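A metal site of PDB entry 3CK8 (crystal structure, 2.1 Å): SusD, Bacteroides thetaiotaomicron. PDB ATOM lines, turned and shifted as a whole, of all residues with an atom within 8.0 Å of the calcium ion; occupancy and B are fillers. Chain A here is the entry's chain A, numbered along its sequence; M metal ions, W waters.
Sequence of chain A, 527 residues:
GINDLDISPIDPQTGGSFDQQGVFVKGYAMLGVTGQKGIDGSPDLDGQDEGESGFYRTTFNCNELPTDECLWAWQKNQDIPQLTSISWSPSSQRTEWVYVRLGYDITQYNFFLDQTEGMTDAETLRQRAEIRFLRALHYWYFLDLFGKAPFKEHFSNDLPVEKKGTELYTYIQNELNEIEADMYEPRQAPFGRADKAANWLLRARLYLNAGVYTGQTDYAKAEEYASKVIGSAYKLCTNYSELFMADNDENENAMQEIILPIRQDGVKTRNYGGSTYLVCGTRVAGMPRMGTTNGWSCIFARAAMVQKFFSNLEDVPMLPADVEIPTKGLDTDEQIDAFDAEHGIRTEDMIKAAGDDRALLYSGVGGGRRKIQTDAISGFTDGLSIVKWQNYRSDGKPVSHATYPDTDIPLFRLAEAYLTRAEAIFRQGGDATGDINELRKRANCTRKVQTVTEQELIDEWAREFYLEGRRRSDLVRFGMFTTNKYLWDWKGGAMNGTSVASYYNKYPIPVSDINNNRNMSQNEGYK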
ATOM      1  N   PHE A 191      -5.785  -1.661 -21.623  1.00  0.00           N
ATOM      2  CA  PHE A 191      -4.967  -2.863 -21.714  1.00  0.00           C
ATOM      3  C   PHE A 191      -4.804  -3.552 -20.367  1.00  0.00           C
ATOM      4  O   PHE A 191      -4.366  -2.937 -19.384  1.00  0.00           O
ATOM      5  CB  PHE A 191      -3.572  -2.532 -22.277  1.00  0.00           C
ATOM      6  CG  PHE A 191      -2.830  -3.744 -22.772  1.00  0.00           C
ATOM      7  CD1 PHE A 191      -3.335  -4.490 -23.831  1.00  0.00           C
ATOM      8  CD2 PHE A 191      -1.637  -4.139 -22.174  1.00  0.00           C
ATOM      9  CE1 PHE A 191      -2.660  -5.624 -24.290  1.00  0.00           C
ATOM     10  CE2 PHE A 191      -0.957  -5.268 -22.617  1.00  0.00           C
ATOM     11  CZ  PHE A 191      -1.479  -6.016 -23.677  1.00  0.00           C
ATOM     12  N   MET A 245       7.885 -11.109 -25.267  1.00  0.00           N
ATOM     13  CA  MET A 245       9.028 -10.267 -24.951  1.00  0.00           C
ATOM     14  C   MET A 245       8.660  -9.140 -23.994  1.00  0.00           C
ATOM     15  O   MET A 245       7.484  -8.894 -23.740  1.00  0.00           O
ATOM     16  CB  MET A 245       9.638  -9.724 -26.244  1.00  0.00           C
ATOM     17  CG  MET A 245      10.325 -10.812 -27.064  1.00  0.00           C
ATOM     18  SD  MET A 245      10.974 -10.266 -28.649  1.00  0.00           S
ATOM     19  CE  MET A 245      12.545  -9.499 -28.139  1.00  0.00           C
ATOM     20  N   ALA A 246       9.678  -8.467 -23.472  1.00  0.00           N
ATOM     21  CA  ALA A 246       9.508  -7.402 -22.490  1.00  0.00           C
ATOM     22  C   ALA A 246       8.585  -6.251 -22.855  1.00  0.00           C
ATOM     23  O   ALA A 246       7.974  -5.636 -21.981  1.00  0.00           O
ATOM     24  CB  ALA A 246      10.876  -6.859 -22.078  1.00  0.00           C
ATOM     25  N   ASP A 247       8.493  -5.938 -24.145  1.00  0.00           N
ATOM     26  CA  ASP A 247       7.640  -4.835 -24.575  1.00  0.00           C
ATOM     27  C   ASP A 247       6.303  -5.270 -25.164  1.00  0.00           C
ATOM     28  O   ASP A 247       5.699  -4.533 -25.952  1.00  0.00           O
ATOM     29  CB  ASP A 247       8.394  -3.961 -25.581  1.00  0.00           C
ATOM     30  CG  ASP A 247       8.838  -4.719 -26.824  1.00  0.00           C
ATOM     31  OD1 ASP A 247       9.076  -5.947 -26.732  1.00  0.00           O
ATOM     32  OD2 ASP A 247       8.984  -4.081 -27.882  1.00  0.00           O
ATOM     33  N   ASN A 248       5.825  -6.458 -24.789  1.00  0.00           N
ATOM     34  CA  ASN A 248       4.556  -6.932 -25.330  1.00  0.00           C
ATOM     35  C   ASN A 248       3.341  -6.156 -24.830  1.00  0.00           C
ATOM     36  O   ASN A 248       2.201  -6.498 -25.157  1.00  0.00           O
ATOM     37  CB  ASN A 248       4.374  -8.447 -25.094  1.00  0.00           C
ATOM     38  CG  ASN A 248       4.378  -8.837 -23.624  1.00  0.00           C
ATOM     39  OD1 ASN A 248       4.364  -7.982 -22.734  1.00  0.00           O
ATOM     40  ND2 ASN A 248       4.389 -10.141 -23.358  1.00  0.00           N
ATOM     41  N   ASP A 249       3.592  -5.092 -24.073  1.00  0.00           N
ATOM     42  CA  ASP A 249       2.518  -4.217 -23.587  1.00  0.00           C
ATOM     43  C   ASP A 249       2.754  -2.793 -24.110  1.00  0.00           C
ATOM     44  O   ASP A 249       2.091  -1.846 -23.691  1.00  0.00           O
ATOM     45  CB  ASP A 249       2.435  -4.205 -22.050  1.00  0.00           C
ATOM     46  CG  ASP A 249       3.688  -3.632 -21.389  1.00  0.00           C
ATOM     47  OD1 ASP A 249       4.594  -3.156 -22.104  1.00  0.00           O
ATOM     48  OD2 ASP A 249       3.739  -3.651 -20.139  1.00  0.00           O
ATOM     49  N   GLU A 250       3.715  -2.668 -25.018  1.00  0.00           N
ATOM     50  CA  GLU A 250       4.034  -1.378 -25.628  1.00  0.00           C
ATOM     51  C   GLU A 250       4.470  -1.618 -27.074  1.00  0.00           C
ATOM     52  O   GLU A 250       5.309  -0.895 -27.624  1.00  0.00           O
ATOM     53  CB  GLU A 250       5.150  -0.672 -24.843  1.00  0.00           C
ATOM     54  CG  GLU A 250       4.794  -0.412 -23.377  1.00  0.00           C
ATOM     55  CD  GLU A 250       5.841   0.402 -22.629  1.00  0.00           C
ATOM     56  OE1 GLU A 250       7.010   0.430 -23.062  1.00  0.00           O
ATOM     57  OE2 GLU A 250       5.490   1.005 -21.602  1.00  0.00           O
ATOM     58  N   PRO A 261      -4.036  -9.917 -21.250  1.00  0.00           N
ATOM     59  CA  PRO A 261      -2.691 -10.092 -20.708  1.00  0.00           C
ATOM     60  C   PRO A 261      -2.726 -10.034 -19.182  1.00  0.00           C
ATOM     61  O   PRO A 261      -3.657  -9.493 -18.593  1.00  0.00           O
ATOM     62  CB  PRO A 261      -1.938  -8.907 -21.292  1.00  0.00           C
ATOM     63  CG  PRO A 261      -2.976  -7.825 -21.155  1.00  0.00           C
ATOM     64  CD  PRO A 261      -4.273  -8.500 -21.586  1.00  0.00           C
ATOM     65  N   ILE A 262      -1.723 -10.618 -18.564  1.00  0.00           N
ATOM     66  CA  ILE A 262      -1.599 -10.575 -17.117  1.00  0.00           C
ATOM     67  C   ILE A 262      -0.439  -9.591 -17.035  1.00  0.00           C
ATOM     68  O   ILE A 262       0.689  -9.924 -17.399  1.00  0.00           O
ATOM     69  CB  ILE A 262      -1.186 -11.936 -16.514  1.00  0.00           C
ATOM     70  CG1 ILE A 262      -2.385 -12.887 -16.543  1.00  0.00           C
ATOM     71  CG2 ILE A 262      -0.705 -11.743 -15.077  1.00  0.00           C
ATOM     72  CD1 ILE A 262      -2.103 -14.264 -15.949  1.00  0.00           C
ATOM     73  N   ARG A 263      -0.722  -8.373 -16.596  1.00  0.00           N
ATOM     74  CA  ARG A 263       0.319  -7.366 -16.522  1.00  0.00           C
ATOM     75  C   ARG A 263       1.410  -7.773 -15.539  1.00  0.00           C
ATOM     76  O   ARG A 263       1.123  -8.221 -14.437  1.00  0.00           O
ATOM     77  CB  ARG A 263      -0.274  -6.008 -16.109  1.00  0.00           C
ATOM     78  CG  ARG A 263      -1.432  -5.518 -16.982  1.00  0.00           C
ATOM     79  CD  ARG A 263      -1.103  -5.567 -18.473  1.00  0.00           C
ATOM     80  NE  ARG A 263       0.043  -4.735 -18.846  1.00  0.00           N
ATOM     81  CZ  ARG A 263       0.033  -3.408 -18.872  1.00  0.00           C
ATOM     82  NH1 ARG A 263      -1.065  -2.739 -18.555  1.00  0.00           N
ATOM     83  NH2 ARG A 263       1.126  -2.752 -19.224  1.00  0.00           N
ATOM     84  N   GLN A 264       2.653  -7.612 -15.967  1.00  0.00           N
ATOM     85  CA  GLN A 264       3.827  -7.905 -15.161  1.00  0.00           C
ATOM     86  C   GLN A 264       4.814  -6.771 -15.425  1.00  0.00           C
ATOM     87  O   GLN A 264       4.905  -6.274 -16.547  1.00  0.00           O
ATOM     88  CB  GLN A 264       4.469  -9.228 -15.595  1.00  0.00           C
ATOM     89  CG  GLN A 264       3.555 -10.434 -15.401  1.00  0.00           C
ATOM     90  CD  GLN A 264       3.522 -10.912 -13.968  1.00  0.00           C
ATOM     91  OE1 GLN A 264       4.343 -11.742 -13.556  1.00  0.00           O
ATOM     92  NE2 GLN A 264       2.589 -10.382 -13.185  1.00  0.00           N
ATOM     93  N   ASP A 265       5.532  -6.354 -14.402  1.00  0.00           N
ATOM     94  CA  ASP A 265       6.500  -5.284 -14.551  1.00  0.00           C
ATOM     95  C   ASP A 265       7.671  -5.548 -13.613  1.00  0.00           C
ATOM     96  O   ASP A 265       7.480  -5.925 -12.451  1.00  0.00           O
ATOM     97  CB  ASP A 265       5.846  -3.934 -14.248  1.00  0.00           C
ATOM     98  CG  ASP A 265       6.787  -2.757 -14.479  1.00  0.00           C
ATOM     99  OD1 ASP A 265       7.498  -2.373 -13.544  1.00  0.00           O
ATOM    100  OD2 ASP A 265       6.817  -2.230 -15.630  1.00  0.00           O
ATOM    101  N   GLY A 266       8.876  -5.352 -14.141  1.00  0.00           N
ATOM    102  CA  GLY A 266      10.081  -5.595 -13.373  1.00  0.00           C
ATOM    103  C   GLY A 266      10.224  -4.855 -12.055  1.00  0.00           C
ATOM    104  O   GLY A 266      10.872  -5.354 -11.141  1.00  0.00           O
ATOM    105  N   LYS A 268       7.337  -2.740 -10.527  1.00  0.00           N
ATOM    106  CA  LYS A 268       6.060  -2.642  -9.820  1.00  0.00           C
ATOM    107  C   LYS A 268       5.287  -3.932  -9.576  1.00  0.00           C
ATOM    108  O   LYS A 268       4.733  -4.147  -8.500  1.00  0.00           O
ATOM    109  CB  LYS A 268       5.127  -1.694 -10.587  1.00  0.00           C
ATOM    110  CG  LYS A 268       5.700  -0.311 -10.877  1.00  0.00           C
ATOM    111  CD  LYS A 268       4.801   0.442 -11.847  1.00  0.00           C
ATOM    112  CE  LYS A 268       4.588  -0.357 -13.143  1.00  0.00           C
ATOM    113  NZ  LYS A 268       3.763   0.354 -14.162  1.00  0.00           N
ATOM    114  N   THR A 269       5.215  -4.787 -10.596  1.00  0.00           N
ATOM    115  CA  THR A 269       4.456  -6.024 -10.507  1.00  0.00           C
ATOM    116  C   THR A 269       5.357  -7.252 -10.592  1.00  0.00           C
ATOM    117  O   THR A 269       5.607  -7.770 -11.677  1.00  0.00           O
ATOM    118  CB  THR A 269       3.407  -6.077 -11.645  1.00  0.00           C
ATOM    119  OG1 THR A 269       2.804  -4.788 -11.789  1.00  0.00           O
ATOM    120  CG2 THR A 269       2.315  -7.090 -11.334  1.00  0.00           C
ATOM    121  N   SER A 275       5.770 -13.919 -14.832  1.00  0.00           N
ATOM    122  CA  SER A 275       6.703 -13.952 -15.948  1.00  0.00           C
ATOM    123  C   SER A 275       8.116 -14.221 -15.423  1.00  0.00           C
ATOM    124  O   SER A 275       8.983 -14.676 -16.157  1.00  0.00           O
ATOM    125  CB  SER A 275       6.668 -12.635 -16.736  1.00  0.00           C
ATOM    126  OG  SER A 275       6.924 -11.521 -15.907  1.00  0.00           O
ATOM    127  N   ASN A 391      13.076 -11.525 -21.482  1.00  0.00           N
ATOM    128  CA  ASN A 391      12.992 -10.237 -20.839  1.00  0.00           C
ATOM    129  C   ASN A 391      13.813  -9.240 -21.639  1.00  0.00           C
ATOM    130  O   ASN A 391      14.670  -8.528 -21.082  1.00  0.00           O
ATOM    131  CB  ASN A 391      13.497 -10.284 -19.398  1.00  0.00           C
ATOM    132  CG  ASN A 391      13.163  -9.007 -18.651  1.00  0.00           C
ATOM    133  OD1 ASN A 391      13.884  -8.599 -17.740  1.00  0.00           O
ATOM    134  ND2 ASN A 391      12.060  -8.373 -19.036  1.00  0.00           N
ATOM    135  N   ARG A 393      13.228  -6.367 -24.934  1.00  0.00           N
ATOM    136  CA  ARG A 393      12.231  -5.650 -25.715  1.00  0.00           C
ATOM    137  C   ARG A 393      12.557  -5.830 -27.196  1.00  0.00           C
ATOM    138  O   ARG A 393      13.732  -5.818 -27.581  1.00  0.00           O
ATOM    139  CB  ARG A 393      12.246  -4.154 -25.384  1.00  0.00           C
ATOM    140  CG  ARG A 393      11.799  -3.791 -23.972  1.00  0.00           C
ATOM    141  CD  ARG A 393      11.902  -2.292 -23.766  1.00  0.00           C
ATOM    142  NE  ARG A 393      11.036  -1.525 -24.675  1.00  0.00           N
ATOM    143  CZ  ARG A 393       9.793  -1.143 -24.385  1.00  0.00           C
ATOM    144  NH1 ARG A 393       9.264  -1.444 -23.207  1.00  0.00           N
ATOM    145  NH2 ARG A 393       9.096  -0.447 -25.263  1.00  0.00           N
ATOM    146  N   SER A 400      12.897  -2.426 -17.282  1.00  0.00           N
ATOM    147  CA  SER A 400      12.933  -1.722 -16.001  1.00  0.00           C
ATOM    148  C   SER A 400      13.808  -2.362 -14.906  1.00  0.00           C
ATOM    149  O   SER A 400      14.279  -1.660 -14.018  1.00  0.00           O
ATOM    150  CB  SER A 400      11.512  -1.558 -15.458  1.00  0.00           C
ATOM    151  OG  SER A 400      11.057  -2.768 -14.855  1.00  0.00           O
ATOM    152  N   PRO A 405      11.492  -9.614 -14.922  1.00  0.00           N
ATOM    153  CA  PRO A 405      11.034  -9.227 -16.269  1.00  0.00           C
ATOM    154  C   PRO A 405       9.823  -8.310 -16.347  1.00  0.00           C
ATOM    155  O   PRO A 405       8.965  -8.299 -15.464  1.00  0.00           O
ATOM    156  CB  PRO A 405      10.770 -10.577 -16.939  1.00  0.00           C
ATOM    157  CG  PRO A 405      10.259 -11.399 -15.806  1.00  0.00           C
ATOM    158  CD  PRO A 405      11.197 -11.045 -14.663  1.00  0.00           C
ATOM    159  N   ASP A 406       9.765  -7.546 -17.436  1.00  0.00           N
ATOM    160  CA  ASP A 406       8.663  -6.648 -17.695  1.00  0.00           C
ATOM    161  C   ASP A 406       7.650  -7.385 -18.548  1.00  0.00           C
ATOM    162  O   ASP A 406       6.517  -6.939 -18.725  1.00  0.00           O
ATOM    163  CB  ASP A 406       9.123  -5.412 -18.466  1.00  0.00           C
ATOM    164  CG  ASP A 406      10.041  -4.526 -17.654  1.00  0.00           C
ATOM    165  OD1 ASP A 406       9.979  -4.572 -16.410  1.00  0.00           O
ATOM    166  OD2 ASP A 406      10.807  -3.755 -18.271  1.00  0.00           O
ATOM    167  N   THR A 407       8.055  -8.534 -19.073  1.00  0.00           N
ATOM    168  CA  THR A 407       7.212  -9.341 -19.946  1.00  0.00           C
ATOM    169  C   THR A 407       5.855  -9.712 -19.357  1.00  0.00           C
ATOM    170  O   THR A 407       5.768 -10.304 -18.289  1.00  0.00           O
ATOM    171  CB  THR A 407       7.936 -10.624 -20.349  1.00  0.00           C
ATOM    172  OG1 THR A 407       9.227 -10.298 -20.889  1.00  0.00           O
ATOM    173  CG2 THR A 407       7.131 -11.388 -21.394  1.00  0.00           C
ATOM    174  N   ASP A 408       4.796  -9.363 -20.086  1.00  0.00           N
ATOM    175  CA  ASP A 408       3.424  -9.678 -19.687  1.00  0.00           C
ATOM    176  C   ASP A 408       3.137 -11.107 -20.128  1.00  0.00           C
ATOM    177  O   ASP A 408       3.762 -11.620 -21.063  1.00  0.00           O
ATOM    178  CB  ASP A 408       2.425  -8.765 -20.396  1.00  0.00           C
ATOM    179  CG  ASP A 408       2.254  -7.423 -19.716  1.00  0.00           C
ATOM    180  OD1 ASP A 408       3.061  -7.073 -18.828  1.00  0.00           O
ATOM    181  OD2 ASP A 408       1.298  -6.704 -20.081  1.00  0.00           O
ATOM    182  N   ILE A 409       2.178 -11.751 -19.469  1.00  0.00           N
ATOM    183  CA  ILE A 409       1.777 -13.093 -19.850  1.00  0.00           C
ATOM    184  C   ILE A 409       0.515 -12.965 -20.690  1.00  0.00           C
ATOM    185  O   ILE A 409      -0.549 -12.599 -20.181  1.00  0.00           O
ATOM    186  CB  ILE A 409       1.448 -13.954 -18.605  1.00  0.00           C
ATOM    187  CG1 ILE A 409       2.716 -14.199 -17.788  1.00  0.00           C
ATOM    188  CG2 ILE A 409       0.832 -15.284 -19.053  1.00  0.00           C
ATOM    189  CD1 ILE A 409       2.467 -14.876 -16.468  1.00  0.00           C
HETATM  190 CA    CA M   1       4.680  -5.394 -18.765  1.00  0.00          CA
HETATM  191  O   HOH W   1       6.460  -3.744 -18.339  1.00  0.00           O
HETATM  192  O   HOH W   2       3.214  -4.023 -17.198  1.00  0.00           O
HETATM  193  O   HOH W   3       5.337  -5.949 -21.090  1.00  0.00           O
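The guanidinium group of Arg 263 is in salt-bridge range of the side-chain carboxylate of Asp 408 (2.6 Å). The backbone carbonyl oxygen of Asp 408 sits at hydrogen-bond distance from the side-chain amide nitrogen of Asn 248, at 2.8 Å. OE1 of Gln 264 is in hydrogen-bond range of N of Ser 275 (2.9 Å). N of Gly 266 sits at hydrogen-bond distance from OD1 of Asp 406 (2.6 Å). The side-chain carboxylate (OD1) of Asp 406 is in hydrogen-bond range of the side-chain hydroxyl (OG) of Ser 400, at 2.6 Å. The backbone NH (N) of Asp 406 lies close to the side-chain amide nitrogen (ND2) of Asn 391. The guanidinium group of Arg 263 lies close to the side-chain carboxylate of Asp 249 (2.9 Å).
Four residues have an atom within 4 Å of the calcium ion: Asp 249, Gln 264, Asp 406 and Asp 408. The nearest printed residue that does not touch the calcium ion is Arg 263 (4.5 Å).
The calcium ion is bound by the side-chain carboxylate of Asp 408, the backbone carbonyl oxygen of Gln 264, the backbone carbonyl oxygen of Asp 406, the side-chain carboxylate of Asp 249, water W1, water W3 and water W2.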
